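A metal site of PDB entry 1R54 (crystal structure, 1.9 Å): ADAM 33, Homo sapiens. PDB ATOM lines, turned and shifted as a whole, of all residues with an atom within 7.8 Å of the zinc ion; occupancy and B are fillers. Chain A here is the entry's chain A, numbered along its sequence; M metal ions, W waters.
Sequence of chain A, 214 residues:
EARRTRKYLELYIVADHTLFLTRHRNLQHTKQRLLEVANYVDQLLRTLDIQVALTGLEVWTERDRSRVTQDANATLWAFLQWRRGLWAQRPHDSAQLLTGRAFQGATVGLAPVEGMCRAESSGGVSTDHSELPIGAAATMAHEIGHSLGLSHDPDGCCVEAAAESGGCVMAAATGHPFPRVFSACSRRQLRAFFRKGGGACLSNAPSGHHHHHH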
ATOM      1  N   GLY A 109      -6.457   0.466  20.503  1.00  0.00           N
ATOM      2  CA  GLY A 109      -7.087  -0.842  20.455  1.00  0.00           C
ATOM      3  C   GLY A 109      -8.092  -0.878  19.319  1.00  0.00           C
ATOM      4  O   GLY A 109      -8.560   0.169  18.880  1.00  0.00           O
ATOM      5  N   LEU A 110      -8.438  -2.074  18.860  1.00  0.00           N
ATOM      6  CA  LEU A 110      -9.398  -2.193  17.754  1.00  0.00           C
ATOM      7  C   LEU A 110     -10.039  -3.573  17.686  1.00  0.00           C
ATOM      8  O   LEU A 110      -9.400  -4.586  17.944  1.00  0.00           O
ATOM      9  CB  LEU A 110      -8.694  -1.893  16.431  1.00  0.00           C
ATOM     10  CG  LEU A 110      -9.562  -1.720  15.182  1.00  0.00           C
ATOM     11  CD1 LEU A 110     -10.403  -0.467  15.322  1.00  0.00           C
ATOM     12  CD2 LEU A 110      -8.671  -1.633  13.947  1.00  0.00           C
ATOM     13  N   VAL A 113     -17.019  -4.385  15.173  1.00  0.00           N
ATOM     14  CA  VAL A 113     -18.250  -4.111  15.907  1.00  0.00           C
ATOM     15  C   VAL A 113     -19.239  -5.262  15.733  1.00  0.00           C
ATOM     16  O   VAL A 113     -19.474  -5.719  14.620  1.00  0.00           O
ATOM     17  CB  VAL A 113     -18.911  -2.796  15.426  1.00  0.00           C
ATOM     18  CG1 VAL A 113     -20.241  -2.587  16.129  1.00  0.00           C
ATOM     19  CG2 VAL A 113     -17.989  -1.608  15.707  1.00  0.00           C
ATOM     20  N   THR A 139      -8.499  -0.967  27.751  1.00  0.00           N
ATOM     21  CA  THR A 139      -8.551  -0.884  26.301  1.00  0.00           C
ATOM     22  C   THR A 139      -9.184  -2.140  25.709  1.00  0.00           C
ATOM     23  O   THR A 139     -10.032  -2.062  24.815  1.00  0.00           O
ATOM     24  CB  THR A 139      -7.141  -0.741  25.706  1.00  0.00           C
ATOM     25  OG1 THR A 139      -6.576   0.510  26.107  1.00  0.00           O
ATOM     26  CG2 THR A 139      -7.174  -0.824  24.187  1.00  0.00           C
ATOM     27  N   HIS A 142     -12.863  -2.305  26.486  1.00  0.00           N
ATOM     28  CA  HIS A 142     -13.567  -1.333  25.635  1.00  0.00           C
ATOM     29  C   HIS A 142     -13.839  -1.975  24.276  1.00  0.00           C
ATOM     30  O   HIS A 142     -14.946  -1.864  23.737  1.00  0.00           O
ATOM     31  CB  HIS A 142     -12.705  -0.077  25.453  1.00  0.00           C
ATOM     32  CG  HIS A 142     -13.320   0.970  24.583  1.00  0.00           C
ATOM     33  ND1 HIS A 142     -14.017   2.052  25.084  1.00  0.00           N
ATOM     34  CD2 HIS A 142     -13.301   1.136  23.232  1.00  0.00           C
ATOM     35  CE1 HIS A 142     -14.400   2.830  24.084  1.00  0.00           C
ATOM     36  NE2 HIS A 142     -13.975   2.299  22.950  1.00  0.00           N
ATOM     37  N   GLU A 143     -12.829  -2.660  23.732  1.00  0.00           N
ATOM     38  CA  GLU A 143     -12.970  -3.322  22.429  1.00  0.00           C
ATOM     39  C   GLU A 143     -13.888  -4.538  22.501  1.00  0.00           C
ATOM     40  O   GLU A 143     -14.568  -4.860  21.533  1.00  0.00           O
ATOM     41  CB  GLU A 143     -11.604  -3.732  21.884  1.00  0.00           C
ATOM     42  CG  GLU A 143     -10.720  -2.555  21.521  1.00  0.00           C
ATOM     43  CD  GLU A 143     -11.444  -1.524  20.677  1.00  0.00           C
ATOM     44  OE1 GLU A 143     -12.079  -1.900  19.679  1.00  0.00           O
ATOM     45  OE2 GLU A 143     -11.389  -0.330  21.024  1.00  0.00           O
ATOM     46  N   GLY A 145     -16.308  -4.584  24.362  1.00  0.00           N
ATOM     47  CA  GLY A 145     -17.583  -3.904  24.428  1.00  0.00           C
ATOM     48  C   GLY A 145     -18.086  -3.651  23.020  1.00  0.00           C
ATOM     49  O   GLY A 145     -19.260  -3.869  22.717  1.00  0.00           O
ATOM     50  N   HIS A 146     -17.198  -3.172  22.150  1.00  0.00           N
ATOM     51  CA  HIS A 146     -17.568  -2.928  20.754  1.00  0.00           C
ATOM     52  C   HIS A 146     -17.942  -4.238  20.093  1.00  0.00           C
ATOM     53  O   HIS A 146     -18.836  -4.284  19.249  1.00  0.00           O
ATOM     54  CB  HIS A 146     -16.406  -2.298  19.986  1.00  0.00           C
ATOM     55  CG  HIS A 146     -16.272  -0.823  20.204  1.00  0.00           C
ATOM     56  ND1 HIS A 146     -17.341   0.041  20.100  1.00  0.00           N
ATOM     57  CD2 HIS A 146     -15.193  -0.059  20.478  1.00  0.00           C
ATOM     58  CE1 HIS A 146     -16.929   1.276  20.316  1.00  0.00           C
ATOM     59  NE2 HIS A 146     -15.634   1.239  20.550  1.00  0.00           N
ATOM     60  N   LEU A 150     -21.631  -2.613  21.884  1.00  0.00           N
ATOM     61  CA  LEU A 150     -21.778  -1.465  22.777  1.00  0.00           C
ATOM     62  C   LEU A 150     -21.199  -0.221  22.122  1.00  0.00           C
ATOM     63  O   LEU A 150     -20.128  -0.264  21.516  1.00  0.00           O
ATOM     64  CB  LEU A 150     -21.085  -1.718  24.111  1.00  0.00           C
ATOM     65  CG  LEU A 150     -21.402  -3.009  24.875  1.00  0.00           C
ATOM     66  CD1 LEU A 150     -20.704  -2.976  26.225  1.00  0.00           C
ATOM     67  CD2 LEU A 150     -22.903  -3.158  25.056  1.00  0.00           C
ATOM     68  N   SER A 151     -21.908   0.897  22.255  1.00  0.00           N
ATOM     69  CA  SER A 151     -21.429   2.149  21.677  1.00  0.00           C
ATOM     70  C   SER A 151     -20.704   2.939  22.752  1.00  0.00           C
ATOM     71  O   SER A 151     -20.662   2.536  23.917  1.00  0.00           O
ATOM     72  CB  SER A 151     -22.610   2.968  21.156  1.00  0.00           C
ATOM     73  OG  SER A 151     -23.377   3.472  22.229  1.00  0.00           O
ATOM     74  N   HIS A 152     -20.129   4.067  22.365  1.00  0.00           N
ATOM     75  CA  HIS A 152     -19.460   4.921  23.326  1.00  0.00           C
ATOM     76  C   HIS A 152     -20.574   5.551  24.151  1.00  0.00           C
ATOM     77  O   HIS A 152     -21.698   5.699  23.669  1.00  0.00           O
ATOM     78  CB  HIS A 152     -18.645   6.009  22.614  1.00  0.00           C
ATOM     79  CG  HIS A 152     -17.392   5.489  21.981  1.00  0.00           C
ATOM     80  ND1 HIS A 152     -16.604   6.261  21.159  1.00  0.00           N
ATOM     81  CD2 HIS A 152     -16.784   4.289  22.071  1.00  0.00           C
ATOM     82  CE1 HIS A 152     -15.554   5.560  20.766  1.00  0.00           C
ATOM     83  NE2 HIS A 152     -15.644   4.349  21.301  1.00  0.00           N
ATOM     84  N   VAL A 169     -15.900   2.455  31.148  1.00  0.00           N
ATOM     85  CA  VAL A 169     -15.157   1.812  30.072  1.00  0.00           C
ATOM     86  C   VAL A 169     -15.461   2.256  28.643  1.00  0.00           C
ATOM     87  O   VAL A 169     -14.544   2.424  27.848  1.00  0.00           O
ATOM     88  CB  VAL A 169     -15.312   0.268  30.158  1.00  0.00           C
ATOM     89  CG1 VAL A 169     -14.544  -0.409  29.022  1.00  0.00           C
ATOM     90  CG2 VAL A 169     -14.791  -0.224  31.507  1.00  0.00           C
ATOM     91  N   MET A 170     -16.733   2.457  28.314  1.00  0.00           N
ATOM     92  CA  MET A 170     -17.063   2.862  26.955  1.00  0.00           C
ATOM     93  C   MET A 170     -16.964   4.368  26.707  1.00  0.00           C
ATOM     94  O   MET A 170     -17.682   4.919  25.880  1.00  0.00           O
ATOM     95  CB  MET A 170     -18.453   2.348  26.574  1.00  0.00           C
ATOM     96  CG  MET A 170     -18.577   0.830  26.524  1.00  0.00           C
ATOM     97  SD  MET A 170     -17.206  -0.010  25.671  1.00  0.00           S
ATOM     98  CE  MET A 170     -17.399   0.588  23.969  1.00  0.00           C
ATOM     99  N   ALA A 171     -16.058   5.031  27.422  1.00  0.00           N
ATOM    100  CA  ALA A 171     -15.836   6.457  27.237  1.00  0.00           C
ATOM    101  C   ALA A 171     -15.085   6.611  25.910  1.00  0.00           C
ATOM    102  O   ALA A 171     -14.320   5.716  25.522  1.00  0.00           O
ATOM    103  CB  ALA A 171     -15.006   7.015  28.376  1.00  0.00           C
ATOM    104  N   ALA A 172     -15.293   7.728  25.234  1.00  0.00           N
ATOM    105  CA  ALA A 172     -14.631   7.967  23.947  1.00  0.00           C
ATOM    106  C   ALA A 172     -13.151   8.304  24.101  1.00  0.00           C
ATOM    107  O   ALA A 172     -12.377   8.109  23.168  1.00  0.00           O
ATOM    108  CB  ALA A 172     -15.341   9.087  23.210  1.00  0.00           C
ATOM    109  N   ALA A 173     -12.767   8.787  25.277  1.00  0.00           N
ATOM    110  CA  ALA A 173     -11.367   9.136  25.535  1.00  0.00           C
ATOM    111  C   ALA A 173     -10.712   8.135  26.471  1.00  0.00           C
ATOM    112  O   ALA A 173     -11.368   7.576  27.360  1.00  0.00           O
ATOM    113  CB  ALA A 173     -11.282  10.536  26.128  1.00  0.00           C
HETATM  114 ZN    ZN M   1     -14.380   2.847  20.892  1.00  0.00          ZN
HETATM  115  O   HOH W   1     -14.690   3.329  18.492  1.00  0.00           O
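ND1 of His 142 sits at hydrogen-bond distance from O of Val 169, at 2.8 Å.
The backbone carbonyl oxygen of Leu 150 sits at hydrogen-bond distance from a ring nitrogen (ND1) of His 146, at 3.1 Å.
The nearest printed residue that does not touch the zinc ion is Glu 143 (4.4 Å).
The zinc ion is bound by a ring nitrogen (NE2) of His 152 (2.0 Å), a ring nitrogen (NE2) of His 146 (2.1 Å), a ring nitrogen (NE2) of His 142 (2.2 Å) and water W1 (2.5 Å).
The zinc ion has four donor atoms within binding distance.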
